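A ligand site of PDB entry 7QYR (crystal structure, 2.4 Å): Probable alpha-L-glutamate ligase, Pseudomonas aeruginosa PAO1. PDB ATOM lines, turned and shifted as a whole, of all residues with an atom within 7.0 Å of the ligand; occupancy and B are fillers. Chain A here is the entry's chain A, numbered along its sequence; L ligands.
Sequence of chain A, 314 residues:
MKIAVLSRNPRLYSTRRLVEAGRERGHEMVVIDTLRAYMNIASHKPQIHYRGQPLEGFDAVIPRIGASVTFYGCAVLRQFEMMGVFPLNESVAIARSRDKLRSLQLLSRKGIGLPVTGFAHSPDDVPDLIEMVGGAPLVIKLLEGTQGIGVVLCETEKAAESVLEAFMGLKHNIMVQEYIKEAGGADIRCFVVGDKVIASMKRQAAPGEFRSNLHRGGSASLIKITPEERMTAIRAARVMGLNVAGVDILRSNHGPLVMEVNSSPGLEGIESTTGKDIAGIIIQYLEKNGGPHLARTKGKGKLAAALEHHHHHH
NZ of Lys 141 lies within hydrogen-bond range of OE1 of Gln 177, 3.1 Å away.
The side-chain hydroxyl of Ser 212 sits at hydrogen-bond distance from the side-chain carboxylate of Asp 187.
O of Asp 248 sits at hydrogen-bond distance from N of Met 259 (2.8 Å).
OE2 of Glu 178 sits at hydrogen-bond distance from N of Val 116 (2.9 Å).
The side-chain carboxylate of Asp 187 lies within salt-bridge range of the guanidinium group of Arg 203.
N of Val 139 sits at hydrogen-bond distance from O of Gln 177 (2.7 Å).
OG of Ser 212 sits at hydrogen-bond distance from O4 of the ligand.
The side-chain amide nitrogen (ND2) of Asn 213 sits at hydrogen-bond distance from an oxygen (O1) of the ligand, 2.9 Å away.
OE1 of Gln 177 sits at hydrogen-bond distance from N3 of the ligand (3.4 Å).
NZ of Lys 141 sits at hydrogen-bond distance from N2 of the ligand.
N3 of the ligand lies within hydrogen-bond range of O of Glu 178, 2.9 Å away.
An oxygen (O3) of the ligand lies within hydrogen-bond range of the side-chain carboxylate of Asp 187 (3.5 Å).
A nitrogen (N4) of the ligand sits at hydrogen-bond distance from the backbone NH (N) of Ile 180, at 3.0 Å.
Val 139 touches the ligand.
Tyr 179 touches the ligand.
O of Phe 210 touches O4 of the ligand, 3.6 Å away.
Arg 211 touches the ligand.
Leu 250 touches the ligand (CD1 to C9, 3.7 Å).
CE of Met 259 touches N2 of the ligand, 3.3 Å away.
Hydrophobic or aromatic side chains that line the ligand: Val 139, Tyr 179, Ile 180, Phe 210, Leu 250 and Met 259.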
ATOM      1  N   PRO A 115      13.343 -20.370 -27.001  1.00  0.00           N
ATOM      2  CA  PRO A 115      14.469 -20.097 -26.115  1.00  0.00           C
ATOM      3  C   PRO A 115      15.468 -19.270 -26.930  1.00  0.00           C
ATOM      4  O   PRO A 115      15.556 -19.476 -28.107  1.00  0.00           O
ATOM      5  CB  PRO A 115      15.024 -21.460 -25.741  1.00  0.00           C
ATOM      6  CG  PRO A 115      13.917 -22.440 -26.117  1.00  0.00           C
ATOM      7  CD  PRO A 115      13.176 -21.809 -27.278  1.00  0.00           C
ATOM      8  N   VAL A 116      16.173 -18.333 -26.302  1.00  0.00           N
ATOM      9  CA  VAL A 116      17.350 -17.679 -26.953  1.00  0.00           C
ATOM     10  C   VAL A 116      18.246 -18.814 -27.475  1.00  0.00           C
ATOM     11  O   VAL A 116      18.534 -19.725 -26.686  1.00  0.00           O
ATOM     12  CB  VAL A 116      18.081 -16.737 -25.974  1.00  0.00           C
ATOM     13  CG1 VAL A 116      19.437 -16.300 -26.534  1.00  0.00           C
ATOM     14  CG2 VAL A 116      17.225 -15.537 -25.603  1.00  0.00           C
ATOM     15  N   LEU A 138      23.481 -23.117 -20.079  1.00  0.00           N
ATOM     16  CA  LEU A 138      22.808 -23.303 -21.375  1.00  0.00           C
ATOM     17  C   LEU A 138      22.740 -24.789 -21.724  1.00  0.00           C
ATOM     18  O   LEU A 138      23.449 -25.582 -21.094  1.00  0.00           O
ATOM     19  CB  LEU A 138      23.488 -22.449 -22.457  1.00  0.00           C
ATOM     20  CG  LEU A 138      25.009 -22.428 -22.452  1.00  0.00           C
ATOM     21  CD1 LEU A 138      25.550 -23.718 -23.019  1.00  0.00           C
ATOM     22  CD2 LEU A 138      25.531 -21.236 -23.249  1.00  0.00           C
ATOM     23  N   VAL A 139      21.820 -25.134 -22.625  1.00  0.00           N
ATOM     24  CA  VAL A 139      21.612 -26.499 -23.175  1.00  0.00           C
ATOM     25  C   VAL A 139      22.323 -26.559 -24.538  1.00  0.00           C
ATOM     26  O   VAL A 139      22.128 -25.655 -25.345  1.00  0.00           O
ATOM     27  CB  VAL A 139      20.113 -26.814 -23.268  1.00  0.00           C
ATOM     28  CG1 VAL A 139      19.846 -28.097 -24.005  1.00  0.00           C
ATOM     29  CG2 VAL A 139      19.519 -26.884 -21.865  1.00  0.00           C
ATOM     30  N   LYS A 141      22.485 -28.925 -27.880  1.00  0.00           N
ATOM     31  CA  LYS A 141      21.855 -29.990 -28.701  1.00  0.00           C
ATOM     32  C   LYS A 141      22.773 -30.287 -29.880  1.00  0.00           C
ATOM     33  O   LYS A 141      23.314 -29.335 -30.505  1.00  0.00           O
ATOM     34  CB  LYS A 141      20.452 -29.565 -29.148  1.00  0.00           C
ATOM     35  CG  LYS A 141      19.482 -29.429 -27.981  1.00  0.00           C
ATOM     36  CD  LYS A 141      18.062 -29.086 -28.277  1.00  0.00           C
ATOM     37  CE  LYS A 141      17.460 -28.234 -27.177  1.00  0.00           C
ATOM     38  NZ  LYS A 141      15.995 -28.135 -27.328  1.00  0.00           N
ATOM     39  N   VAL A 151      21.311 -34.106 -25.988  1.00  0.00           N
ATOM     40  CA  VAL A 151      20.885 -32.849 -25.300  1.00  0.00           C
ATOM     41  C   VAL A 151      21.595 -32.821 -23.951  1.00  0.00           C
ATOM     42  O   VAL A 151      21.501 -33.802 -23.201  1.00  0.00           O
ATOM     43  CB  VAL A 151      19.365 -32.806 -25.142  1.00  0.00           C
ATOM     44  CG1 VAL A 151      18.876 -31.456 -24.654  1.00  0.00           C
ATOM     45  CG2 VAL A 151      18.643 -33.218 -26.414  1.00  0.00           C
ATOM     46  N   LEU A 153      23.047 -30.409 -20.514  1.00  0.00           N
ATOM     47  CA  LEU A 153      23.068 -29.221 -19.639  1.00  0.00           C
ATOM     48  C   LEU A 153      24.531 -28.897 -19.330  1.00  0.00           C
ATOM     49  O   LEU A 153      25.257 -29.763 -18.822  1.00  0.00           O
ATOM     50  CB  LEU A 153      22.272 -29.537 -18.374  1.00  0.00           C
ATOM     51  CG  LEU A 153      22.214 -28.415 -17.350  1.00  0.00           C
ATOM     52  CD1 LEU A 153      21.624 -27.141 -17.978  1.00  0.00           C
ATOM     53  CD2 LEU A 153      21.488 -28.874 -16.095  1.00  0.00           C
ATOM     54  N   GLN A 177      21.312 -23.171 -26.482  1.00  0.00           N
ATOM     55  CA  GLN A 177      20.030 -22.580 -26.007  1.00  0.00           C
ATOM     56  C   GLN A 177      20.159 -22.166 -24.539  1.00  0.00           C
ATOM     57  O   GLN A 177      20.768 -22.897 -23.766  1.00  0.00           O
ATOM     58  CB  GLN A 177      18.864 -23.567 -26.116  1.00  0.00           C
ATOM     59  CG  GLN A 177      18.358 -23.754 -27.541  1.00  0.00           C
ATOM     60  CD  GLN A 177      16.982 -24.366 -27.586  1.00  0.00           C
ATOM     61  OE1 GLN A 177      16.625 -25.202 -26.765  1.00  0.00           O
ATOM     62  NE2 GLN A 177      16.192 -23.900 -28.538  1.00  0.00           N
ATOM     63  N   GLU A 178      19.529 -21.063 -24.148  1.00  0.00           N
ATOM     64  CA  GLU A 178      19.330 -20.696 -22.726  1.00  0.00           C
ATOM     65  C   GLU A 178      18.647 -21.884 -22.044  1.00  0.00           C
ATOM     66  O   GLU A 178      17.761 -22.504 -22.672  1.00  0.00           O
ATOM     67  CB  GLU A 178      18.563 -19.377 -22.582  1.00  0.00           C
ATOM     68  CG  GLU A 178      17.124 -19.453 -23.032  1.00  0.00           C
ATOM     69  CD  GLU A 178      16.278 -18.220 -22.724  1.00  0.00           C
ATOM     70  OE1 GLU A 178      16.570 -17.537 -21.715  1.00  0.00           O
ATOM     71  OE2 GLU A 178      15.366 -17.898 -23.509  1.00  0.00           O
ATOM     72  N   TYR A 179      19.105 -22.224 -20.834  1.00  0.00           N
ATOM     73  CA  TYR A 179      18.484 -23.230 -19.937  1.00  0.00           C
ATOM     74  C   TYR A 179      17.276 -22.576 -19.272  1.00  0.00           C
ATOM     75  O   TYR A 179      17.439 -21.579 -18.567  1.00  0.00           O
ATOM     76  CB  TYR A 179      19.481 -23.753 -18.898  1.00  0.00           C
ATOM     77  CG  TYR A 179      18.924 -24.759 -17.920  1.00  0.00           C
ATOM     78  CD1 TYR A 179      18.147 -25.824 -18.353  1.00  0.00           C
ATOM     79  CD2 TYR A 179      19.183 -24.660 -16.568  1.00  0.00           C
ATOM     80  CE1 TYR A 179      17.635 -26.760 -17.476  1.00  0.00           C
ATOM     81  CE2 TYR A 179      18.716 -25.620 -15.673  1.00  0.00           C
ATOM     82  CZ  TYR A 179      17.946 -26.675 -16.131  1.00  0.00           C
ATOM     83  OH  TYR A 179      17.476 -27.621 -15.270  1.00  0.00           O
ATOM     84  N   ILE A 180      16.087 -23.124 -19.507  1.00  0.00           N
ATOM     85  CA  ILE A 180      14.807 -22.710 -18.861  1.00  0.00           C
ATOM     86  C   ILE A 180      14.688 -23.491 -17.547  1.00  0.00           C
ATOM     87  O   ILE A 180      13.914 -24.469 -17.498  1.00  0.00           O
ATOM     88  CB  ILE A 180      13.625 -22.920 -19.815  1.00  0.00           C
ATOM     89  CG1 ILE A 180      13.877 -22.330 -21.214  1.00  0.00           C
ATOM     90  CG2 ILE A 180      12.378 -22.321 -19.190  1.00  0.00           C
ATOM     91  CD1 ILE A 180      14.260 -20.816 -21.211  1.00  0.00           C
ATOM     92  N   LYS A 181      15.390 -23.063 -16.496  1.00  0.00           N
ATOM     93  CA  LYS A 181      15.367 -23.709 -15.161  1.00  0.00           C
ATOM     94  C   LYS A 181      13.962 -23.610 -14.558  1.00  0.00           C
ATOM     95  O   LYS A 181      13.557 -24.561 -13.856  1.00  0.00           O
ATOM     96  CB  LYS A 181      16.401 -23.101 -14.204  1.00  0.00           C
ATOM     97  CG  LYS A 181      16.512 -23.850 -12.893  1.00  0.00           C
ATOM     98  CD  LYS A 181      17.530 -23.281 -11.964  1.00  0.00           C
ATOM     99  CE  LYS A 181      17.022 -22.074 -11.194  1.00  0.00           C
ATOM    100  NZ  LYS A 181      18.041 -21.521 -10.272  1.00  0.00           N
ATOM    101  N   ALA A 183      11.086 -23.943 -15.622  1.00  0.00           N
ATOM    102  CA  ALA A 183      10.174 -25.025 -16.076  1.00  0.00           C
ATOM    103  C   ALA A 183      10.212 -26.211 -15.092  1.00  0.00           C
ATOM    104  O   ALA A 183       9.283 -27.021 -15.148  1.00  0.00           O
ATOM    105  CB  ALA A 183      10.539 -25.471 -17.470  1.00  0.00           C
ATOM    106  N   GLY A 185      11.892 -29.003 -15.035  1.00  0.00           N
ATOM    107  CA  GLY A 185      11.949 -30.334 -15.680  1.00  0.00           C
ATOM    108  C   GLY A 185      10.618 -30.752 -16.319  1.00  0.00           C
ATOM    109  O   GLY A 185      10.507 -31.915 -16.740  1.00  0.00           O
ATOM    110  N   ALA A 186       9.633 -29.854 -16.392  1.00  0.00           N
ATOM    111  CA  ALA A 186       8.310 -30.106 -17.021  1.00  0.00           C
ATOM    112  C   ALA A 186       8.276 -29.469 -18.415  1.00  0.00           C
ATOM    113  O   ALA A 186       8.960 -28.456 -18.633  1.00  0.00           O
ATOM    114  CB  ALA A 186       7.209 -29.535 -16.147  1.00  0.00           C
ATOM    115  N   ASP A 187       7.515 -30.073 -19.336  1.00  0.00           N
ATOM    116  CA  ASP A 187       7.157 -29.483 -20.640  1.00  0.00           C
ATOM    117  C   ASP A 187       5.685 -29.804 -20.927  1.00  0.00           C
ATOM    118  O   ASP A 187       5.131 -30.704 -20.291  1.00  0.00           O
ATOM    119  CB  ASP A 187       8.113 -29.919 -21.750  1.00  0.00           C
ATOM    120  CG  ASP A 187       7.900 -31.343 -22.263  1.00  0.00           C
ATOM    121  OD1 ASP A 187       7.522 -32.211 -21.430  1.00  0.00           O
ATOM    122  OD2 ASP A 187       8.163 -31.596 -23.443  1.00  0.00           O
ATOM    123  N   ARG A 203       4.452 -33.328 -19.155  1.00  0.00           N
ATOM    124  CA  ARG A 203       5.479 -34.380 -18.947  1.00  0.00           C
ATOM    125  C   ARG A 203       6.500 -33.864 -17.921  1.00  0.00           C
ATOM    126  O   ARG A 203       7.069 -32.804 -18.158  1.00  0.00           O
ATOM    127  CB  ARG A 203       6.141 -34.738 -20.277  1.00  0.00           C
ATOM    128  CG  ARG A 203       5.322 -35.669 -21.157  1.00  0.00           C
ATOM    129  CD  ARG A 203       5.464 -35.369 -22.640  1.00  0.00           C
ATOM    130  NE  ARG A 203       6.832 -35.146 -23.075  1.00  0.00           N
ATOM    131  CZ  ARG A 203       7.201 -34.915 -24.335  1.00  0.00           C
ATOM    132  NH1 ARG A 203       8.482 -34.736 -24.614  1.00  0.00           N
ATOM    133  NH2 ARG A 203       6.299 -34.834 -25.293  1.00  0.00           N
ATOM    134  N   ALA A 205      10.029 -34.780 -15.890  1.00  0.00           N
ATOM    135  CA  ALA A 205      11.275 -35.586 -15.810  1.00  0.00           C
ATOM    136  C   ALA A 205      11.447 -36.082 -14.365  1.00  0.00           C
ATOM    137  O   ALA A 205      11.067 -35.342 -13.451  1.00  0.00           O
ATOM    138  CB  ALA A 205      12.467 -34.763 -16.233  1.00  0.00           C
ATOM    139  N   PHE A 210      16.921 -33.637 -16.284  1.00  0.00           N
ATOM    140  CA  PHE A 210      16.258 -32.403 -16.783  1.00  0.00           C
ATOM    141  C   PHE A 210      15.466 -32.741 -18.058  1.00  0.00           C
ATOM    142  O   PHE A 210      14.448 -32.074 -18.319  1.00  0.00           O
ATOM    143  CB  PHE A 210      17.280 -31.275 -16.994  1.00  0.00           C
ATOM    144  CG  PHE A 210      17.894 -31.247 -18.370  1.00  0.00           C
ATOM    145  CD1 PHE A 210      17.353 -30.461 -19.370  1.00  0.00           C
ATOM    146  CD2 PHE A 210      18.975 -32.061 -18.695  1.00  0.00           C
ATOM    147  CE1 PHE A 210      17.871 -30.470 -20.653  1.00  0.00           C
ATOM    148  CE2 PHE A 210      19.480 -32.088 -19.982  1.00  0.00           C
ATOM    149  CZ  PHE A 210      18.926 -31.285 -20.962  1.00  0.00           C
ATOM    150  N   ARG A 211      15.944 -33.729 -18.846  1.00  0.00           N
ATOM    151  CA  ARG A 211      15.311 -34.208 -20.098  1.00  0.00           C
ATOM    152  C   ARG A 211      14.069 -35.030 -19.728  1.00  0.00           C
ATOM    153  O   ARG A 211      14.228 -36.000 -18.960  1.00  0.00           O
ATOM    154  CB  ARG A 211      16.320 -34.997 -20.940  1.00  0.00           C
ATOM    155  N   SER A 212      12.888 -34.652 -20.229  1.00  0.00           N
ATOM    156  CA  SER A 212      11.559 -35.016 -19.662  1.00  0.00           C
ATOM    157  C   SER A 212      10.766 -35.961 -20.564  1.00  0.00           C
ATOM    158  O   SER A 212       9.541 -36.023 -20.378  1.00  0.00           O
ATOM    159  CB  SER A 212      10.732 -33.773 -19.329  1.00  0.00           C
ATOM    160  OG  SER A 212      10.207 -33.182 -20.504  1.00  0.00           O
ATOM    161  N   ASN A 213      11.431 -36.661 -21.494  1.00  0.00           N
ATOM    162  CA  ASN A 213      10.749 -37.604 -22.420  1.00  0.00           C
ATOM    163  C   ASN A 213      10.094 -38.725 -21.582  1.00  0.00           C
ATOM    164  O   ASN A 213      10.720 -39.149 -20.585  1.00  0.00           O
ATOM    165  CB  ASN A 213      11.705 -38.164 -23.488  1.00  0.00           C
ATOM    166  CG  ASN A 213      12.289 -37.105 -24.412  1.00  0.00           C
ATOM    167  OD1 ASN A 213      11.886 -36.984 -25.557  1.00  0.00           O
ATOM    168  ND2 ASN A 213      13.273 -36.356 -23.931  1.00  0.00           N
ATOM    169  N   ASP A 248       5.736 -29.178 -28.447  1.00  0.00           N
ATOM    170  CA  ASP A 248       6.289 -29.236 -27.075  1.00  0.00           C
ATOM    171  C   ASP A 248       6.611 -27.807 -26.680  1.00  0.00           C
ATOM    172  O   ASP A 248       7.265 -27.072 -27.463  1.00  0.00           O
ATOM    173  CB  ASP A 248       7.511 -30.161 -27.012  1.00  0.00           C
ATOM    174  CG  ASP A 248       7.197 -31.637 -27.250  1.00  0.00           C
ATOM    175  OD1 ASP A 248       6.024 -32.042 -27.030  1.00  0.00           O
ATOM    176  OD2 ASP A 248       8.131 -32.378 -27.615  1.00  0.00           O
ATOM    177  N   LEU A 250       7.856 -25.148 -23.336  1.00  0.00           N
ATOM    178  CA  LEU A 250       8.390 -24.867 -21.982  1.00  0.00           C
ATOM    179  C   LEU A 250       7.741 -23.590 -21.442  1.00  0.00           C
ATOM    180  O   LEU A 250       7.673 -22.594 -22.182  1.00  0.00           O
ATOM    181  CB  LEU A 250       9.908 -24.672 -22.062  1.00  0.00           C
ATOM    182  CG  LEU A 250      10.715 -25.949 -22.257  1.00  0.00           C
ATOM    183  CD1 LEU A 250      12.208 -25.585 -22.280  1.00  0.00           C
ATOM    184  CD2 LEU A 250      10.389 -27.014 -21.185  1.00  0.00           C
ATOM    185  N   MET A 259       9.741 -25.891 -28.190  1.00  0.00           N
ATOM    186  CA  MET A 259      10.986 -26.712 -28.180  1.00  0.00           C
ATOM    187  C   MET A 259      11.020 -27.599 -29.426  1.00  0.00           C
ATOM    188  O   MET A 259      12.100 -27.760 -30.010  1.00  0.00           O
ATOM    189  CB  MET A 259      11.029 -27.625 -26.950  1.00  0.00           C
ATOM    190  CG  MET A 259      10.972 -26.877 -25.643  1.00  0.00           C
ATOM    191  SD  MET A 259      12.077 -25.400 -25.602  1.00  0.00           S
ATOM    192  CE  MET A 259      13.636 -26.196 -25.915  1.00  0.00           C
ATOM    193  N   GLU A 260       9.880 -28.157 -29.796  1.00  0.00           N
ATOM    194  CA  GLU A 260       9.741 -29.211 -30.828  1.00  0.00           C
ATOM    195  C   GLU A 260       8.419 -29.006 -31.561  1.00  0.00           C
ATOM    196  O   GLU A 260       7.422 -28.695 -30.906  1.00  0.00           O
ATOM    197  CB  GLU A 260       9.807 -30.587 -30.149  1.00  0.00           C
ATOM    198  CG  GLU A 260      10.016 -31.741 -31.112  1.00  0.00           C
ATOM    199  CD  GLU A 260      11.309 -31.643 -31.900  1.00  0.00           C
ATOM    200  OE1 GLU A 260      12.390 -31.874 -31.299  1.00  0.00           O
ATOM    201  OE2 GLU A 260      11.233 -31.300 -33.106  1.00  0.00           O
HETATM  202  O1  LIG L   1      14.677 -34.008 -25.012  1.00  0.00           O
HETATM  203  C1  LIG L   1      14.532 -32.576 -24.752  1.00  0.00           C
HETATM  204  C2  LIG L   1      13.942 -32.362 -23.369  1.00  0.00           C
HETATM  205  O2  LIG L   1      14.898 -31.632 -22.562  1.00  0.00           O
HETATM  206  C3  LIG L   1      12.631 -31.550 -23.321  1.00  0.00           C
HETATM  207  O3  LIG L   1      11.522 -32.417 -23.157  1.00  0.00           O
HETATM  208  C4  LIG L   1      12.792 -30.629 -22.103  1.00  0.00           C
HETATM  209  O4  LIG L   1      12.217 -31.148 -20.927  1.00  0.00           O
HETATM  210  C5  LIG L   1      14.311 -30.496 -21.947  1.00  0.00           C
HETATM  211  N1  LIG L   1      14.881 -29.298 -22.545  1.00  0.00           N
HETATM  212  C6  LIG L   1      15.289 -29.132 -23.839  1.00  0.00           C
HETATM  213  N2  LIG L   1      15.771 -27.933 -24.103  1.00  0.00           N
HETATM  214  C7  LIG L   1      15.677 -27.270 -22.883  1.00  0.00           C
HETATM  215  C8  LIG L   1      16.035 -25.963 -22.507  1.00  0.00           C
HETATM  216  N3  LIG L   1      16.572 -25.080 -23.345  1.00  0.00           N
HETATM  217  N4  LIG L   1      15.822 -25.611 -21.215  1.00  0.00           N
HETATM  218  C9  LIG L   1      15.279 -26.521 -20.390  1.00  0.00           C
HETATM  219  N5  LIG L   1      14.899 -27.776 -20.638  1.00  0.00           N
HETATM  220  C10 LIG L   1      15.133 -28.100 -21.920  1.00  0.00           C
